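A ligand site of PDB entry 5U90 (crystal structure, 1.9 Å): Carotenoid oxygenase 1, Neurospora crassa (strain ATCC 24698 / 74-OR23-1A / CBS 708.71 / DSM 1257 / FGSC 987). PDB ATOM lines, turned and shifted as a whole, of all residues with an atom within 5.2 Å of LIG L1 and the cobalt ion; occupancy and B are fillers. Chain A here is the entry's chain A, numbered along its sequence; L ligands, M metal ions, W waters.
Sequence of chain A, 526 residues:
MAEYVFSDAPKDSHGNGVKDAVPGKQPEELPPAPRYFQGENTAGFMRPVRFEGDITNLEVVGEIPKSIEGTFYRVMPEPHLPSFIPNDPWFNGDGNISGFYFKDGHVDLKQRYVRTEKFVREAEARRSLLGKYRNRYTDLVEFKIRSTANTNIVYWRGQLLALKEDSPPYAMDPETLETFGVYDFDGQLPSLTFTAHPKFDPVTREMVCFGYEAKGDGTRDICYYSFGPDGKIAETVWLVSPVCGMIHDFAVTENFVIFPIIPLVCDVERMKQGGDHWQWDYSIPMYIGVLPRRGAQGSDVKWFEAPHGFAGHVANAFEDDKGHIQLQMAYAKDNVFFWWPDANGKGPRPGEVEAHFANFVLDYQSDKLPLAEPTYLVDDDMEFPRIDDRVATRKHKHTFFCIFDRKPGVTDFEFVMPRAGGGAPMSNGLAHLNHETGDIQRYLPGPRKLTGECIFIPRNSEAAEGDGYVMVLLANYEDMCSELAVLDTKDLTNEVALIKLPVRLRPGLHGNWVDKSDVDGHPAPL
The cobalt ion is bound by a ring nitrogen (NE2) of His 313 (2.1 Å), a ring nitrogen (NE2) of His 197 (2.1 Å), a ring nitrogen (NE2) of His 510 (2.2 Å), a ring nitrogen (NE2) of His 248 (2.2 Å) and water W3 (2.3 Å).
Merely in contact with LIG L1: Phe 91 (3.4 Å), Thr 151 (3.5 Å), Glu 165 (3.3 Å), Phe 310 (3.8 Å), Gly 312 (3.4 Å), Phe 337 (3.6 Å), Phe 384 (3.2 Å) and Pro 425 (3.6 Å).
Hydrophobic or aromatic side chains that line LIG L1: Phe 91, Tyr 133, His 248, Phe 310, His 313, Phe 337, Phe 384 and Pro 425.
Of the 20 residues printed, 13 come within 4 Å of LIG L1.
Water W1 bridges the backbone carbonyl oxygen (O) of Ala 311 (2.8 Å) and an oxygen (O3) of LIG L1 (2.9 Å).
O1 of LG2 L2 lies within hydrogen-bond range of O2 of LIG L1, at 2.7 Å.
An oxygen (O3) of LIG L1 lies within hydrogen-bond range of a ring nitrogen (ND1) of His 313.
The side-chain hydroxyl (OH) of Tyr 133 lies within hydrogen-bond range of an oxygen (O1) of LIG L1, 2.5 Å away.
NZ of Lys 164 lies within hydrogen-bond range of O1 of LIG L1, at 2.6 Å.
OE2 of Glu 383 lies within hydrogen-bond range of O3 of LIG L1 (2.7 Å).
ND1 of His 313 lies within hydrogen-bond range of OE1 of Glu 383 (2.7 Å).
The backbone carbonyl oxygen (O) of Thr 151 is in hydrogen-bond range of the backbone NH (N) of His 510 (3.1 Å).
ND1 of His 248 lies within hydrogen-bond range of OE2 of Glu 165.
NZ of Lys 164 lies within hydrogen-bond range of O of Phe 91 (2.9 Å).
OD1 of Asn 150 is in hydrogen-bond range of NZ of Lys 164 (3.0 Å).
The backbone carbonyl oxygen of Phe 91 lies within hydrogen-bond range of the side-chain amide nitrogen of Asn 150, 2.9 Å away.
The side-chain hydroxyl (OG1) of Thr 151 is in hydrogen-bond range of the side-chain amide oxygen (OD1) of Asn 150 (2.7 Å).
Within 4 Å of the cobalt ion: His 197, His 248, His 313 and His 510.
Along chain A the residues within 4 Å of the cobalt ion span positions 197 to 510.
The nearest printed residue that does not touch the cobalt ion is Thr 151 (4.6 Å).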
ATOM      1  N   PHE A  91      -6.859  -3.115 -15.832  1.00  0.00           N
ATOM      2  CA  PHE A  91      -6.710  -1.671 -15.859  1.00  0.00           C
ATOM      3  C   PHE A  91      -6.418  -1.103 -17.244  1.00  0.00           C
ATOM      4  O   PHE A  91      -6.511   0.125 -17.403  1.00  0.00           O
ATOM      5  CB  PHE A  91      -5.610  -1.120 -14.910  1.00  0.00           C
ATOM      6  CG  PHE A  91      -5.777  -1.432 -13.461  1.00  0.00           C
ATOM      7  CD1 PHE A  91      -7.002  -1.844 -12.895  1.00  0.00           C
ATOM      8  CD2 PHE A  91      -4.660  -1.324 -12.618  1.00  0.00           C
ATOM      9  CE1 PHE A  91      -7.096  -2.147 -11.549  1.00  0.00           C
ATOM     10  CE2 PHE A  91      -4.759  -1.608 -11.270  1.00  0.00           C
ATOM     11  CZ  PHE A  91      -5.955  -2.041 -10.729  1.00  0.00           C
ATOM     12  N   TYR A 133       0.244  -1.835 -20.709  1.00  0.00           N
ATOM     13  CA  TYR A 133      -0.205  -0.809 -19.775  1.00  0.00           C
ATOM     14  C   TYR A 133       0.915   0.212 -19.539  1.00  0.00           C
ATOM     15  O   TYR A 133       2.004  -0.132 -19.037  1.00  0.00           O
ATOM     16  CB  TYR A 133      -0.633  -1.439 -18.444  1.00  0.00           C
ATOM     17  CG  TYR A 133      -1.147  -0.415 -17.456  1.00  0.00           C
ATOM     18  CD1 TYR A 133      -2.426   0.132 -17.583  1.00  0.00           C
ATOM     19  CD2 TYR A 133      -0.351   0.057 -16.423  1.00  0.00           C
ATOM     20  CE1 TYR A 133      -2.906   1.124 -16.710  1.00  0.00           C
ATOM     21  CE2 TYR A 133      -0.784   1.007 -15.528  1.00  0.00           C
ATOM     22  CZ  TYR A 133      -2.085   1.551 -15.677  1.00  0.00           C
ATOM     23  OH  TYR A 133      -2.497   2.531 -14.815  1.00  0.00           O
ATOM     24  N   ASN A 150     -10.916   5.084 -18.185  1.00  0.00           N
ATOM     25  CA  ASN A 150     -11.637   3.922 -17.708  1.00  0.00           C
ATOM     26  C   ASN A 150     -11.755   3.774 -16.221  1.00  0.00           C
ATOM     27  O   ASN A 150     -12.222   2.752 -15.751  1.00  0.00           O
ATOM     28  CB  ASN A 150     -10.975   2.658 -18.294  1.00  0.00           C
ATOM     29  CG  ASN A 150      -9.644   2.331 -17.621  1.00  0.00           C
ATOM     30  OD1 ASN A 150      -9.099   3.123 -16.819  1.00  0.00           O
ATOM     31  ND2 ASN A 150      -9.122   1.160 -17.940  1.00  0.00           N
ATOM     32  N   THR A 151     -11.377   4.798 -15.468  1.00  0.00           N
ATOM     33  CA  THR A 151     -11.205   4.639 -14.034  1.00  0.00           C
ATOM     34  C   THR A 151     -12.231   5.353 -13.175  1.00  0.00           C
ATOM     35  O   THR A 151     -12.691   4.781 -12.199  1.00  0.00           O
ATOM     36  CB  THR A 151      -9.764   5.094 -13.626  1.00  0.00           C
ATOM     37  OG1 THR A 151      -8.829   4.336 -14.394  1.00  0.00           O
ATOM     38  CG2 THR A 151      -9.536   4.841 -12.138  1.00  0.00           C
ATOM     39  N   LYS A 164      -8.514   9.124 -16.151  1.00  0.00           N
ATOM     40  CA  LYS A 164      -7.481   8.116 -16.224  1.00  0.00           C
ATOM     41  C   LYS A 164      -6.129   8.771 -15.869  1.00  0.00           C
ATOM     42  O   LYS A 164      -5.740   9.747 -16.501  1.00  0.00           O
ATOM     43  CB  LYS A 164      -7.469   7.518 -17.604  1.00  0.00           C
ATOM     44  CG  LYS A 164      -6.400   6.478 -17.883  1.00  0.00           C
ATOM     45  CD  LYS A 164      -6.593   5.257 -17.083  1.00  0.00           C
ATOM     46  CE  LYS A 164      -5.549   4.231 -17.473  1.00  0.00           C
ATOM     47  NZ  LYS A 164      -6.151   2.932 -16.984  1.00  0.00           N
ATOM     48  N   GLU A 165      -5.477   8.260 -14.836  1.00  0.00           N
ATOM     49  CA  GLU A 165      -4.388   8.977 -14.131  1.00  0.00           C
ATOM     50  C   GLU A 165      -3.114   9.239 -14.950  1.00  0.00           C
ATOM     51  O   GLU A 165      -2.234   9.953 -14.456  1.00  0.00           O
ATOM     52  CB  GLU A 165      -4.044   8.243 -12.830  1.00  0.00           C
ATOM     53  CG  GLU A 165      -3.383   6.885 -12.989  1.00  0.00           C
ATOM     54  CD  GLU A 165      -3.535   6.037 -11.754  1.00  0.00           C
ATOM     55  OE1 GLU A 165      -2.454   5.565 -11.232  1.00  0.00           O
ATOM     56  OE2 GLU A 165      -4.678   5.814 -11.300  1.00  0.00           O
ATOM     57  N   HIS A 197      -9.101  10.597  -8.873  1.00  0.00           N
ATOM     58  CA  HIS A 197      -9.783  10.885  -7.614  1.00  0.00           C
ATOM     59  C   HIS A 197      -9.731  12.363  -7.183  1.00  0.00           C
ATOM     60  O   HIS A 197      -9.287  12.674  -6.095  1.00  0.00           O
ATOM     61  CB  HIS A 197      -9.258   9.971  -6.529  1.00  0.00           C
ATOM     62  CG  HIS A 197      -9.624   8.544  -6.741  1.00  0.00           C
ATOM     63  ND1 HIS A 197     -10.919   8.111  -6.563  1.00  0.00           N
ATOM     64  CD2 HIS A 197      -8.926   7.487  -7.217  1.00  0.00           C
ATOM     65  CE1 HIS A 197     -11.003   6.832  -6.884  1.00  0.00           C
ATOM     66  NE2 HIS A 197      -9.799   6.431  -7.282  1.00  0.00           N
ATOM     67  N   MET A 246       3.473   5.268  -7.716  1.00  0.00           N
ATOM     68  CA  MET A 246       2.059   5.399  -8.098  1.00  0.00           C
ATOM     69  C   MET A 246       1.276   6.101  -6.991  1.00  0.00           C
ATOM     70  O   MET A 246       1.209   5.607  -5.852  1.00  0.00           O
ATOM     71  CB  MET A 246       1.472   4.026  -8.394  1.00  0.00           C
ATOM     72  CG  MET A 246      -0.031   4.065  -8.707  1.00  0.00           C
ATOM     73  SD  MET A 246      -0.861   2.475  -8.721  1.00  0.00           S
ATOM     74  CE  MET A 246      -0.375   1.899 -10.322  1.00  0.00           C
ATOM     75  N   HIS A 248      -2.362   6.807  -6.628  1.00  0.00           N
ATOM     76  CA  HIS A 248      -3.662   6.551  -7.210  1.00  0.00           C
ATOM     77  C   HIS A 248      -4.782   7.447  -6.657  1.00  0.00           C
ATOM     78  O   HIS A 248      -5.681   7.875  -7.400  1.00  0.00           O
ATOM     79  CB  HIS A 248      -4.070   5.111  -6.978  1.00  0.00           C
ATOM     80  CG  HIS A 248      -5.372   4.797  -7.602  1.00  0.00           C
ATOM     81  ND1 HIS A 248      -5.546   4.886  -8.967  1.00  0.00           N
ATOM     82  CD2 HIS A 248      -6.578   4.510  -7.082  1.00  0.00           C
ATOM     83  CE1 HIS A 248      -6.807   4.655  -9.268  1.00  0.00           C
ATOM     84  NE2 HIS A 248      -7.447   4.406  -8.147  1.00  0.00           N
ATOM     85  N   PHE A 310       0.575  -0.994   1.091  1.00  0.00           N
ATOM     86  CA  PHE A 310      -0.148  -0.567  -0.116  1.00  0.00           C
ATOM     87  C   PHE A 310      -1.149   0.521   0.284  1.00  0.00           C
ATOM     88  O   PHE A 310      -2.005   0.304   1.132  1.00  0.00           O
ATOM     89  CB  PHE A 310      -0.882  -1.760  -0.734  1.00  0.00           C
ATOM     90  CG  PHE A 310      -1.491  -1.478  -2.060  1.00  0.00           C
ATOM     91  CD1 PHE A 310      -2.783  -0.937  -2.169  1.00  0.00           C
ATOM     92  CD2 PHE A 310      -0.790  -1.740  -3.218  1.00  0.00           C
ATOM     93  CE1 PHE A 310      -3.314  -0.641  -3.422  1.00  0.00           C
ATOM     94  CE2 PHE A 310      -1.325  -1.466  -4.468  1.00  0.00           C
ATOM     95  CZ  PHE A 310      -2.577  -0.916  -4.563  1.00  0.00           C
ATOM     96  N   ALA A 311      -1.024   1.676  -0.346  1.00  0.00           N
ATOM     97  CA  ALA A 311      -1.964   2.791  -0.155  1.00  0.00           C
ATOM     98  C   ALA A 311      -3.230   2.550  -1.009  1.00  0.00           C
ATOM     99  O   ALA A 311      -3.232   2.784  -2.218  1.00  0.00           O
ATOM    100  CB  ALA A 311      -1.323   4.113  -0.574  1.00  0.00           C
ATOM    101  N   GLY A 312      -4.264   2.057  -0.367  1.00  0.00           N
ATOM    102  CA  GLY A 312      -5.573   1.838  -1.013  1.00  0.00           C
ATOM    103  C   GLY A 312      -6.439   3.094  -1.006  1.00  0.00           C
ATOM    104  O   GLY A 312      -5.959   4.166  -0.694  1.00  0.00           O
ATOM    105  N   HIS A 313      -7.723   2.953  -1.344  1.00  0.00           N
ATOM    106  CA  HIS A 313      -8.568   4.136  -1.479  1.00  0.00           C
ATOM    107  C   HIS A 313      -8.794   4.905  -0.190  1.00  0.00           C
ATOM    108  O   HIS A 313      -8.930   4.325   0.896  1.00  0.00           O
ATOM    109  CB  HIS A 313      -9.900   3.794  -2.110  1.00  0.00           C
ATOM    110  CG  HIS A 313      -9.793   3.487  -3.556  1.00  0.00           C
ATOM    111  ND1 HIS A 313      -9.844   2.205  -4.071  1.00  0.00           N
ATOM    112  CD2 HIS A 313      -9.592   4.310  -4.614  1.00  0.00           C
ATOM    113  CE1 HIS A 313      -9.713   2.255  -5.383  1.00  0.00           C
ATOM    114  NE2 HIS A 313      -9.552   3.517  -5.734  1.00  0.00           N
ATOM    115  N   VAL A 336      -1.025  -5.373  -3.461  1.00  0.00           N
ATOM    116  CA  VAL A 336      -2.361  -5.709  -3.956  1.00  0.00           C
ATOM    117  C   VAL A 336      -2.313  -5.994  -5.463  1.00  0.00           C
ATOM    118  O   VAL A 336      -3.028  -6.881  -5.966  1.00  0.00           O
ATOM    119  CB  VAL A 336      -3.377  -4.578  -3.606  1.00  0.00           C
ATOM    120  CG1 VAL A 336      -4.727  -4.773  -4.298  1.00  0.00           C
ATOM    121  CG2 VAL A 336      -3.569  -4.551  -2.088  1.00  0.00           C
ATOM    122  N   PHE A 337      -1.473  -5.252  -6.196  1.00  0.00           N
ATOM    123  CA  PHE A 337      -1.339  -5.429  -7.625  1.00  0.00           C
ATOM    124  C   PHE A 337      -0.185  -6.405  -7.903  1.00  0.00           C
ATOM    125  O   PHE A 337       0.870  -6.068  -8.484  1.00  0.00           O
ATOM    126  CB  PHE A 337      -1.127  -4.075  -8.349  1.00  0.00           C
ATOM    127  CG  PHE A 337      -2.195  -3.020  -8.104  1.00  0.00           C
ATOM    128  CD1 PHE A 337      -3.448  -3.319  -7.594  1.00  0.00           C
ATOM    129  CD2 PHE A 337      -1.909  -1.707  -8.428  1.00  0.00           C
ATOM    130  CE1 PHE A 337      -4.390  -2.301  -7.377  1.00  0.00           C
ATOM    131  CE2 PHE A 337      -2.838  -0.684  -8.228  1.00  0.00           C
ATOM    132  CZ  PHE A 337      -4.085  -0.993  -7.710  1.00  0.00           C
ATOM    133  N   GLU A 383     -12.468  -2.519   0.849  1.00  0.00           N
ATOM    134  CA  GLU A 383     -12.005  -1.520  -0.131  1.00  0.00           C
ATOM    135  C   GLU A 383     -13.203  -0.708  -0.628  1.00  0.00           C
ATOM    136  O   GLU A 383     -14.360  -0.914  -0.168  1.00  0.00           O
ATOM    137  CB  GLU A 383     -11.235  -2.165  -1.322  1.00  0.00           C
ATOM    138  CG  GLU A 383      -9.728  -1.882  -1.310  1.00  0.00           C
ATOM    139  CD  GLU A 383      -9.308  -0.493  -1.735  1.00  0.00           C
ATOM    140  OE1 GLU A 383     -10.180   0.369  -2.058  1.00  0.00           O
ATOM    141  OE2 GLU A 383      -8.056  -0.239  -1.786  1.00  0.00           O
ATOM    142  N   PHE A 384     -12.921   0.234  -1.518  1.00  0.00           N
ATOM    143  CA  PHE A 384     -13.910   1.087  -2.174  1.00  0.00           C
ATOM    144  C   PHE A 384     -14.835   1.794  -1.187  1.00  0.00           C
ATOM    145  O   PHE A 384     -16.058   1.667  -1.276  1.00  0.00           O
ATOM    146  CB  PHE A 384     -14.694   0.256  -3.224  1.00  0.00           C
ATOM    147  CG  PHE A 384     -13.807  -0.668  -4.008  1.00  0.00           C
ATOM    148  CD1 PHE A 384     -12.693  -0.161  -4.689  1.00  0.00           C
ATOM    149  CD2 PHE A 384     -14.050  -2.051  -4.014  1.00  0.00           C
ATOM    150  CE1 PHE A 384     -11.855  -1.033  -5.396  1.00  0.00           C
ATOM    151  CE2 PHE A 384     -13.214  -2.896  -4.686  1.00  0.00           C
ATOM    152  CZ  PHE A 384     -12.120  -2.382  -5.381  1.00  0.00           C
ATOM    153  N   PRO A 425     -10.897  -7.376  -8.566  1.00  0.00           N
ATOM    154  CA  PRO A 425     -11.118  -7.708  -7.168  1.00  0.00           C
ATOM    155  C   PRO A 425     -12.539  -8.210  -6.937  1.00  0.00           C
ATOM    156  O   PRO A 425     -13.418  -7.891  -7.686  1.00  0.00           O
ATOM    157  CB  PRO A 425     -10.915  -6.383  -6.461  1.00  0.00           C
ATOM    158  CG  PRO A 425     -11.347  -5.388  -7.493  1.00  0.00           C
ATOM    159  CD  PRO A 425     -10.843  -5.927  -8.780  1.00  0.00           C
ATOM    160  N   LEU A 509     -14.853  -0.007 -12.334  1.00  0.00           N
ATOM    161  CA  LEU A 509     -14.100   0.775 -11.401  1.00  0.00           C
ATOM    162  C   LEU A 509     -15.076   1.731 -10.753  1.00  0.00           C
ATOM    163  O   LEU A 509     -16.045   1.256 -10.109  1.00  0.00           O
ATOM    164  CB  LEU A 509     -12.884   1.404 -12.081  1.00  0.00           C
ATOM    165  CG  LEU A 509     -11.790   0.364 -12.405  1.00  0.00           C
ATOM    166  CD1 LEU A 509     -10.742   0.861 -13.366  1.00  0.00           C
ATOM    167  CD2 LEU A 509     -11.131  -0.108 -11.121  1.00  0.00           C
ATOM    168  N   HIS A 510     -14.874   3.032 -10.857  1.00  0.00           N
ATOM    169  CA  HIS A 510     -15.601   3.958  -9.985  1.00  0.00           C
ATOM    170  C   HIS A 510     -16.904   4.455 -10.611  1.00  0.00           C
ATOM    171  O   HIS A 510     -17.095   4.317 -11.827  1.00  0.00           O
ATOM    172  CB  HIS A 510     -14.704   5.111  -9.578  1.00  0.00           C
ATOM    173  CG  HIS A 510     -13.556   4.679  -8.756  1.00  0.00           C
ATOM    174  ND1 HIS A 510     -13.711   4.210  -7.475  1.00  0.00           N
ATOM    175  CD2 HIS A 510     -12.243   4.526  -9.059  1.00  0.00           C
ATOM    176  CE1 HIS A 510     -12.538   3.830  -7.012  1.00  0.00           C
ATOM    177  NE2 HIS A 510     -11.647   3.994  -7.964  1.00  0.00           N
HETATM  178  C1  LIG L   1      -7.295   0.131  -5.175  1.00  0.00           C
HETATM  179  C2  LIG L   1      -7.971  -1.087  -5.064  1.00  0.00           C
HETATM  180  C3  LIG L   1      -8.431  -1.718  -6.223  1.00  0.00           C
HETATM  181  C4  LIG L   1      -8.238  -1.150  -7.458  1.00  0.00           C
HETATM  182  C5  LIG L   1      -7.547   0.064  -7.588  1.00  0.00           C
HETATM  183  C6  LIG L   1      -7.083   0.717  -6.431  1.00  0.00           C
HETATM  184  C7  LIG L   1      -7.276   0.522  -8.970  1.00  0.00           C
HETATM  185  C8  LIG L   1      -6.405   1.352  -9.354  1.00  0.00           C
HETATM  186  C9  LIG L   1      -6.124   1.771 -10.739  1.00  0.00           C
HETATM  187  C10 LIG L   1      -7.019   1.576 -11.799  1.00  0.00           C
HETATM  188  C11 LIG L   1      -6.669   1.902 -13.104  1.00  0.00           C
HETATM  189  C12 LIG L   1      -5.415   2.447 -13.365  1.00  0.00           C
HETATM  190  C13 LIG L   1      -4.536   2.669 -12.321  1.00  0.00           C
HETATM  191  C14 LIG L   1      -4.901   2.331 -11.030  1.00  0.00           C
HETATM  192  O1  LIG L   1      -5.026   2.728 -14.644  1.00  0.00           O
HETATM  193  O2  LIG L   1      -9.049  -2.928  -6.152  1.00  0.00           O
HETATM  194  O3  LIG L   1      -6.829   0.742  -4.018  1.00  0.00           O
HETATM  195  C1  LG2 L   2      -6.820 -14.301 -10.848  1.00  0.00           C
HETATM  196  C2  LG2 L   2      -6.189 -14.449 -12.076  1.00  0.00           C
HETATM  197  C3  LG2 L   2      -5.680 -13.316 -12.715  1.00  0.00           C
HETATM  198  C4  LG2 L   2      -5.802 -12.066 -12.125  1.00  0.00           C
HETATM  199  C5  LG2 L   2      -6.434 -11.911 -10.875  1.00  0.00           C
HETATM  200  C6  LG2 L   2      -6.942 -13.053 -10.236  1.00  0.00           C
HETATM  201  C7  LG2 L   2      -6.580 -10.552 -10.288  1.00  0.00           C
HETATM  202  C8  LG2 L   2      -7.038 -10.184  -9.040  1.00  0.00           C
HETATM  203  C9  LG2 L   2      -7.156  -8.767  -8.547  1.00  0.00           C
HETATM  204  C10 LG2 L   2      -7.052  -7.706  -9.442  1.00  0.00           C
HETATM  205  C11 LG2 L   2      -7.151  -6.390  -9.044  1.00  0.00           C
HETATM  206  C12 LG2 L   2      -7.355  -6.098  -7.707  1.00  0.00           C
HETATM  207  C13 LG2 L   2      -7.463  -7.122  -6.777  1.00  0.00           C
HETATM  208  C14 LG2 L   2      -7.362  -8.446  -7.198  1.00  0.00           C
HETATM  209  O1  LG2 L   2      -7.443  -4.786  -7.336  1.00  0.00           O
HETATM  210  O2  LG2 L   2      -5.074 -13.441 -13.931  1.00  0.00           O
HETATM  211  O3  LG2 L   2      -7.322 -15.410 -10.224  1.00  0.00           O
HETATM  212 CO    CO M   1      -9.560   4.386  -7.604  1.00  0.00          CO
HETATM  213  O   HOH W   1      -5.272   3.143  -4.061  1.00  0.00           O
HETATM  214  O   HOH W   2      -9.063  -4.102  -3.983  1.00  0.00           O
HETATM  215  O   HOH W   3      -9.653   2.605  -9.075  1.00  0.00           O
